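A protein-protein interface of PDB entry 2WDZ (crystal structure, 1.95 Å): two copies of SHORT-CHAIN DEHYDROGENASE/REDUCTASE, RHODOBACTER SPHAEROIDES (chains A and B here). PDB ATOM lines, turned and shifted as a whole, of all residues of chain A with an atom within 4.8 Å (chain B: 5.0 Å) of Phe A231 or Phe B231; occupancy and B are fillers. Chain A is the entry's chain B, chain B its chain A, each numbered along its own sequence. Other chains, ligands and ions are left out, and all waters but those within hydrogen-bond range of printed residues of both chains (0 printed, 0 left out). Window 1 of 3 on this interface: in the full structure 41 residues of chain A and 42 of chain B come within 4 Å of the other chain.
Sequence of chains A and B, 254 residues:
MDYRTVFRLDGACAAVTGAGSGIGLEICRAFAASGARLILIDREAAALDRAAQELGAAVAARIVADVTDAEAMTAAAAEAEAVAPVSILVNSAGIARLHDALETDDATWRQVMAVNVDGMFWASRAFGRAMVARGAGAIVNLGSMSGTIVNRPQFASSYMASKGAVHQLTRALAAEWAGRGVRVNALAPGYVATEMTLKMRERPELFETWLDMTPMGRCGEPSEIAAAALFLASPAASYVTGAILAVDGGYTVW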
ATOM      1  N   PHE A   7     -17.067  13.251  -9.828  1.00  0.00           N
ATOM      2  CA  PHE A   7     -17.924  13.128 -11.006  1.00  0.00           C
ATOM      3  C   PHE A   7     -18.543  11.700 -11.254  1.00  0.00           C
ATOM      4  O   PHE A   7     -19.294  11.475 -12.237  1.00  0.00           O
ATOM      5  CB  PHE A   7     -17.165  13.560 -12.217  1.00  0.00           C
ATOM      6  CG  PHE A   7     -16.777  15.005 -12.211  1.00  0.00           C
ATOM      7  CD1 PHE A   7     -17.694  15.981 -12.623  1.00  0.00           C
ATOM      8  CD2 PHE A   7     -15.470  15.378 -11.877  1.00  0.00           C
ATOM      9  CE1 PHE A   7     -17.325  17.309 -12.675  1.00  0.00           C
ATOM     10  CE2 PHE A   7     -15.089  16.710 -11.928  1.00  0.00           C
ATOM     11  CZ  PHE A   7     -16.026  17.684 -12.337  1.00  0.00           C
ATOM     12  N   ALA A 227     -21.930  13.647 -21.167  1.00  0.00           N
ATOM     13  CA  ALA A 227     -20.977  14.259 -20.247  1.00  0.00           C
ATOM     14  C   ALA A 227     -21.608  15.407 -19.438  1.00  0.00           C
ATOM     15  O   ALA A 227     -21.419  15.512 -18.184  1.00  0.00           O
ATOM     16  CB  ALA A 227     -19.732  14.708 -21.026  1.00  0.00           C
ATOM     17  N   ALA A 228     -22.433  16.205 -20.106  1.00  0.00           N
ATOM     18  CA  ALA A 228     -23.123  17.289 -19.415  1.00  0.00           C
ATOM     19  C   ALA A 228     -24.153  16.713 -18.408  1.00  0.00           C
ATOM     20  O   ALA A 228     -24.289  17.213 -17.285  1.00  0.00           O
ATOM     21  CB  ALA A 228     -23.793  18.201 -20.396  1.00  0.00           C
ATOM     22  N   ALA A 229     -24.869  15.653 -18.811  1.00  0.00           N
ATOM     23  CA  ALA A 229     -25.875  15.027 -17.927  1.00  0.00           C
ATOM     24  C   ALA A 229     -25.154  14.398 -16.737  1.00  0.00           C
ATOM     25  O   ALA A 229     -25.639  14.433 -15.625  1.00  0.00           O
ATOM     26  CB  ALA A 229     -26.628  13.961 -18.684  1.00  0.00           C
ATOM     27  N   LEU A 230     -23.991  13.805 -17.028  1.00  0.00           N
ATOM     28  CA  LEU A 230     -23.193  13.133 -16.017  1.00  0.00           C
ATOM     29  C   LEU A 230     -22.847  14.141 -14.964  1.00  0.00           C
ATOM     30  O   LEU A 230     -23.149  13.927 -13.791  1.00  0.00           O
ATOM     31  CB  LEU A 230     -21.967  12.467 -16.613  1.00  0.00           C
ATOM     32  CG  LEU A 230     -20.945  11.787 -15.717  1.00  0.00           C
ATOM     33  CD1 LEU A 230     -21.683  10.875 -14.732  1.00  0.00           C
ATOM     34  CD2 LEU A 230     -19.955  10.957 -16.630  1.00  0.00           C
ATOM     35  N   PHE A 231     -22.348  15.293 -15.402  1.00  0.00           N
ATOM     36  CA  PHE A 231     -22.066  16.413 -14.504  1.00  0.00           C
ATOM     37  C   PHE A 231     -23.260  16.808 -13.625  1.00  0.00           C
ATOM     38  O   PHE A 231     -23.159  16.801 -12.417  1.00  0.00           O
ATOM     39  CB  PHE A 231     -21.555  17.673 -15.255  1.00  0.00           C
ATOM     40  CG  PHE A 231     -21.545  18.910 -14.384  1.00  0.00           C
ATOM     41  CD1 PHE A 231     -20.805  18.939 -13.177  1.00  0.00           C
ATOM     42  CD2 PHE A 231     -22.356  19.982 -14.677  1.00  0.00           C
ATOM     43  CE1 PHE A 231     -20.828  20.045 -12.316  1.00  0.00           C
ATOM     44  CE2 PHE A 231     -22.372  21.133 -13.809  1.00  0.00           C
ATOM     45  CZ  PHE A 231     -21.592  21.154 -12.632  1.00  0.00           C
ATOM     46  N   LEU A 232     -24.382  17.091 -14.270  1.00  0.00           N
ATOM     47  CA  LEU A 232     -25.613  17.487 -13.535  1.00  0.00           C
ATOM     48  C   LEU A 232     -26.128  16.432 -12.535  1.00  0.00           C
ATOM     49  O   LEU A 232     -26.668  16.805 -11.498  1.00  0.00           O
ATOM     50  CB  LEU A 232     -26.717  17.881 -14.489  1.00  0.00           C
ATOM     51  CG  LEU A 232     -26.455  19.210 -15.220  1.00  0.00           C
ATOM     52  CD1 LEU A 232     -27.651  19.410 -16.101  1.00  0.00           C
ATOM     53  CD2 LEU A 232     -26.303  20.448 -14.322  1.00  0.00           C
ATOM     54  N   ALA A 233     -25.973  15.138 -12.887  1.00  0.00           N
ATOM     55  CA  ALA A 233     -26.511  14.051 -12.077  1.00  0.00           C
ATOM     56  C   ALA A 233     -25.577  13.661 -10.962  1.00  0.00           C
ATOM     57  O   ALA A 233     -26.024  13.015 -10.033  1.00  0.00           O
ATOM     58  CB  ALA A 233     -26.838  12.833 -12.918  1.00  0.00           C
ATOM     59  N   SER A 234     -24.302  14.042 -11.058  1.00  0.00           N
ATOM     60  CA  SER A 234     -23.291  13.675 -10.029  1.00  0.00           C
ATOM     61  C   SER A 234     -23.205  14.629  -8.812  1.00  0.00           C
ATOM     62  O   SER A 234     -23.644  15.770  -8.890  1.00  0.00           O
ATOM     63  CB  SER A 234     -21.921  13.663 -10.706  1.00  0.00           C
ATOM     64  OG  SER A 234     -21.395  14.994 -10.677  1.00  0.00           O
ATOM     65  N   ALA A 236     -20.786  16.504  -8.116  1.00  0.00           N
ATOM     66  CA  ALA A 236     -20.140  17.740  -8.562  1.00  0.00           C
ATOM     67  C   ALA A 236     -21.130  18.908  -8.708  1.00  0.00           C
ATOM     68  O   ALA A 236     -20.728  20.064  -8.625  1.00  0.00           O
ATOM     69  CB  ALA A 236     -19.391  17.505  -9.917  1.00  0.00           C
ATOM     70  N   ALA A 237     -22.400  18.596  -8.967  1.00  0.00           N
ATOM     71  CA  ALA A 237     -23.410  19.616  -9.245  1.00  0.00           C
ATOM     72  C   ALA A 237     -24.243  19.916  -7.994  1.00  0.00           C
ATOM     73  O   ALA A 237     -25.412  20.371  -8.089  1.00  0.00           O
ATOM     74  CB  ALA A 237     -24.305  19.169 -10.340  1.00  0.00           C
ATOM     75  N   VAL A 240     -26.202  23.008  -7.702  1.00  0.00           N
ATOM     76  CA  VAL A 240     -26.839  23.323  -8.975  1.00  0.00           C
ATOM     77  C   VAL A 240     -28.261  22.761  -8.981  1.00  0.00           C
ATOM     78  O   VAL A 240     -28.465  21.533  -9.069  1.00  0.00           O
ATOM     79  CB  VAL A 240     -26.041  22.789 -10.211  1.00  0.00           C
ATOM     80  CG1 VAL A 240     -26.720  23.268 -11.562  1.00  0.00           C
ATOM     81  CG2 VAL A 240     -24.610  23.218 -10.184  1.00  0.00           C
ATOM     82  N   LEU A 245     -29.077  24.084 -18.579  1.00  0.00           N
ATOM     83  CA  LEU A 245     -27.686  24.108 -19.046  1.00  0.00           C
ATOM     84  C   LEU A 245     -27.595  23.996 -20.578  1.00  0.00           C
ATOM     85  O   LEU A 245     -27.897  22.942 -21.159  1.00  0.00           O
ATOM     86  CB  LEU A 245     -26.858  23.034 -18.365  1.00  0.00           C
ATOM     87  CG  LEU A 245     -25.456  22.687 -18.929  1.00  0.00           C
ATOM     88  CD1 LEU A 245     -24.560  23.914 -18.895  1.00  0.00           C
ATOM     89  CD2 LEU A 245     -24.814  21.597 -18.097  1.00  0.00           C
ATOM     90  N   PHE B   7     -13.417  14.492 -17.514  1.00  0.00           N
ATOM     91  CA  PHE B   7     -13.371  15.706 -16.725  1.00  0.00           C
ATOM     92  C   PHE B   7     -11.933  16.077 -16.305  1.00  0.00           C
ATOM     93  O   PHE B   7     -11.760  17.008 -15.558  1.00  0.00           O
ATOM     94  CB  PHE B   7     -14.270  15.577 -15.449  1.00  0.00           C
ATOM     95  CG  PHE B   7     -15.700  15.227 -15.752  1.00  0.00           C
ATOM     96  CD1 PHE B   7     -16.612  16.195 -16.163  1.00  0.00           C
ATOM     97  CD2 PHE B   7     -16.115  13.914 -15.679  1.00  0.00           C
ATOM     98  CE1 PHE B   7     -17.941  15.852 -16.480  1.00  0.00           C
ATOM     99  CE2 PHE B   7     -17.471  13.543 -15.964  1.00  0.00           C
ATOM    100  CZ  PHE B   7     -18.380  14.525 -16.372  1.00  0.00           C
ATOM    101  N   ALA B 227     -15.991  22.738  -8.619  1.00  0.00           N
ATOM    102  CA  ALA B 227     -16.351  21.522  -9.400  1.00  0.00           C
ATOM    103  C   ALA B 227     -16.997  21.921 -10.756  1.00  0.00           C
ATOM    104  O   ALA B 227     -16.716  21.320 -11.835  1.00  0.00           O
ATOM    105  CB  ALA B 227     -17.281  20.573  -8.602  1.00  0.00           C
ATOM    106  N   ALA B 228     -17.820  22.957 -10.706  1.00  0.00           N
ATOM    107  CA  ALA B 228     -18.530  23.435 -11.934  1.00  0.00           C
ATOM    108  C   ALA B 228     -17.620  24.157 -12.910  1.00  0.00           C
ATOM    109  O   ALA B 228     -17.850  24.063 -14.125  1.00  0.00           O
ATOM    110  CB  ALA B 228     -19.726  24.309 -11.647  1.00  0.00           C
ATOM    111  N   ALA B 229     -16.659  24.927 -12.385  1.00  0.00           N
ATOM    112  CA  ALA B 229     -15.612  25.476 -13.261  1.00  0.00           C
ATOM    113  C   ALA B 229     -14.812  24.372 -13.931  1.00  0.00           C
ATOM    114  O   ALA B 229     -14.508  24.466 -15.115  1.00  0.00           O
ATOM    115  CB  ALA B 229     -14.732  26.446 -12.551  1.00  0.00           C
ATOM    116  N   LEU B 230     -14.476  23.320 -13.191  1.00  0.00           N
ATOM    117  CA  LEU B 230     -13.771  22.188 -13.763  1.00  0.00           C
ATOM    118  C   LEU B 230     -14.517  21.567 -14.955  1.00  0.00           C
ATOM    119  O   LEU B 230     -13.934  21.331 -16.040  1.00  0.00           O
ATOM    120  CB  LEU B 230     -13.481  21.151 -12.668  1.00  0.00           C
ATOM    121  CG  LEU B 230     -12.756  19.849 -12.971  1.00  0.00           C
ATOM    122  CD1 LEU B 230     -11.482  20.048 -13.786  1.00  0.00           C
ATOM    123  CD2 LEU B 230     -12.388  19.240 -11.635  1.00  0.00           C
ATOM    124  N   PHE B 231     -15.815  21.324 -14.771  1.00  0.00           N
ATOM    125  CA  PHE B 231     -16.613  20.876 -15.888  1.00  0.00           C
ATOM    126  C   PHE B 231     -16.454  21.794 -17.111  1.00  0.00           C
ATOM    127  O   PHE B 231     -16.218  21.328 -18.232  1.00  0.00           O
ATOM    128  CB  PHE B 231     -18.090  20.713 -15.491  1.00  0.00           C
ATOM    129  CG  PHE B 231     -19.049  20.615 -16.697  1.00  0.00           C
ATOM    130  CD1 PHE B 231     -19.057  19.479 -17.528  1.00  0.00           C
ATOM    131  CD2 PHE B 231     -19.922  21.670 -16.997  1.00  0.00           C
ATOM    132  CE1 PHE B 231     -19.915  19.398 -18.635  1.00  0.00           C
ATOM    133  CE2 PHE B 231     -20.796  21.602 -18.116  1.00  0.00           C
ATOM    134  CZ  PHE B 231     -20.791  20.457 -18.934  1.00  0.00           C
ATOM    135  N   LEU B 232     -16.688  23.095 -16.942  1.00  0.00           N
ATOM    136  CA  LEU B 232     -16.672  24.026 -18.096  1.00  0.00           C
ATOM    137  C   LEU B 232     -15.320  24.075 -18.811  1.00  0.00           C
ATOM    138  O   LEU B 232     -15.217  24.339 -20.040  1.00  0.00           O
ATOM    139  CB  LEU B 232     -17.050  25.419 -17.643  1.00  0.00           C
ATOM    140  CG  LEU B 232     -18.506  25.584 -17.172  1.00  0.00           C
ATOM    141  CD1 LEU B 232     -18.833  27.002 -16.573  1.00  0.00           C
ATOM    142  CD2 LEU B 232     -19.486  25.217 -18.322  1.00  0.00           C
ATOM    143  N   ALA B 233     -14.280  23.927 -17.998  1.00  0.00           N
ATOM    144  CA  ALA B 233     -12.944  24.043 -18.476  1.00  0.00           C
ATOM    145  C   ALA B 233     -12.542  22.746 -19.139  1.00  0.00           C
ATOM    146  O   ALA B 233     -11.673  22.763 -19.962  1.00  0.00           O
ATOM    147  CB  ALA B 233     -11.963  24.332 -17.302  1.00  0.00           C
ATOM    148  N   SER B 234     -13.146  21.621 -18.774  1.00  0.00           N
ATOM    149  CA  SER B 234     -12.686  20.315 -19.298  1.00  0.00           C
ATOM    150  C   SER B 234     -13.268  19.885 -20.658  1.00  0.00           C
ATOM    151  O   SER B 234     -14.294  20.414 -21.093  1.00  0.00           O
ATOM    152  CB  SER B 234     -12.996  19.206 -18.310  1.00  0.00           C
ATOM    153  OG  SER B 234     -14.367  19.002 -18.265  1.00  0.00           O
ATOM    154  N   ALA B 236     -15.166  17.544 -21.063  1.00  0.00           N
ATOM    155  CA  ALA B 236     -16.582  17.175 -20.793  1.00  0.00           C
ATOM    156  C   ALA B 236     -17.489  18.242 -21.408  1.00  0.00           C
ATOM    157  O   ALA B 236     -18.547  17.952 -21.936  1.00  0.00           O
ATOM    158  CB  ALA B 236     -16.840  17.086 -19.286  1.00  0.00           C
ATOM    159  N   ALA B 237     -17.041  19.489 -21.370  1.00  0.00           N
ATOM    160  CA  ALA B 237     -17.892  20.600 -21.854  1.00  0.00           C
ATOM    161  C   ALA B 237     -17.611  20.999 -23.298  1.00  0.00           C
ATOM    162  O   ALA B 237     -17.706  22.188 -23.622  1.00  0.00           O
ATOM    163  CB  ALA B 237     -17.764  21.819 -20.909  1.00  0.00           C
ATOM    164  N   VAL B 240     -20.320  23.028 -25.220  1.00  0.00           N
ATOM    165  CA  VAL B 240     -20.834  24.082 -24.414  1.00  0.00           C
ATOM    166  C   VAL B 240     -19.950  25.311 -24.677  1.00  0.00           C
ATOM    167  O   VAL B 240     -18.807  25.325 -24.285  1.00  0.00           O
ATOM    168  CB  VAL B 240     -20.697  23.729 -22.920  1.00  0.00           C
ATOM    169  CG1 VAL B 240     -21.196  24.897 -22.048  1.00  0.00           C
ATOM    170  CG2 VAL B 240     -21.323  22.371 -22.572  1.00  0.00           C
ATOM    171  N   LEU B 245     -23.889  29.270 -16.728  1.00  0.00           N
ATOM    172  CA  LEU B 245     -24.313  28.172 -15.882  1.00  0.00           C
ATOM    173  C   LEU B 245     -24.632  28.639 -14.427  1.00  0.00           C
ATOM    174  O   LEU B 245     -23.716  28.967 -13.668  1.00  0.00           O
ATOM    175  CB  LEU B 245     -23.218  27.076 -15.822  1.00  0.00           C
ATOM    176  CG  LEU B 245     -23.428  25.926 -14.800  1.00  0.00           C
ATOM    177  CD1 LEU B 245     -24.781  25.164 -15.000  1.00  0.00           C
ATOM    178  CD2 LEU B 245     -22.229  24.917 -14.752  1.00  0.00           C
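The backbone carbonyl oxygen (O) of Leu B230 lies close to the side-chain hydroxyl (OG) of Ser B234 (3.2 Å). The backbone carbonyl oxygen (O) of Phe B231 lies within hydrogen-bond range of the side-chain hydroxyl (OG) of Ser B234, 3.0 Å away. The backbone NH (N) of Ala B236 lies close to the side-chain hydroxyl (OG) of Ser B234, at 3.3 Å. The backbone carbonyl oxygen (O) of Phe A231 is in hydrogen-bond range of the side-chain hydroxyl (OG) of Ser A234. The side-chain hydroxyl of Ser A234 lies within hydrogen-bond range of the backbone NH of Ala A236, at 3.0 Å.
Among the printed residues, merely in contact across the chains: Ala A236 with Ala B227 (3.5 Å), Ala A227 with Ala B236 (3.6 Å), Phe A7 with Phe B7 (3.6 Å), Leu A230 with Phe B7 (3.6 Å), Ala A227 with Phe B7 (3.7 Å), Phe A7 with Leu B230 (3.7 Å), Phe A7 with Ala B227 (3.7 Å), Phe A231 with Phe B231 (3.8 Å), Phe A231 with Ala B228 (3.8 Å), Phe A231 with Leu B245 (3.9 Å) and Ala A228 with Phe B231 (3.9 Å).
Of the printed residues of chain A, Leu B245 touches Phe A231 (3.9 Å). Printed residues of chain B within 4 Å of Ala A236: Ala B227 (3.5 Å). Of the printed residues of chain B, Ala A228 touches Phe B231 (3.9 Å). Of the printed residues of chain B, Ala A227 touches Phe B7 and Ala B236. Printed residues of chain A within 4 Å of Ala B227: Phe A7 and Ala A236. Ala A233 touches none of the printed residues of chain B. The nearest printed residue of chain A that does not touch Leu B230 is Phe A231 (7.0 Å).
Of the 13 printed residues of chain A, 6 touch a printed residue of chain B. Hydrophobic or aromatic side chains of chain A that line the printed part of chain B: Phe A7, Ala A227, Leu A230, Phe A231 and Ala A236. Of the 13 printed residues of chain B, 7 touch a printed residue of chain A. Hydrophobic or aromatic side chains of chain B within 4 Å of the printed part of chain A: Phe B7, Ala B227, Ala B228, Leu B230, Phe B231 and Leu B245.
Phe A7 touches its own counterpart, Phe B7. Ala A227 touches Ala B236, and with the chains exchanged Ala A236 touches Ala B227. Ala A228 touches Phe B231, and with the chains exchanged Phe A231 touches Ala B228. Phe B231 touches its own counterpart, Phe A231. Of the 11 pairs that touch across the chains among the printed residues, 10 have their exchanged pair printed and touching as well.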
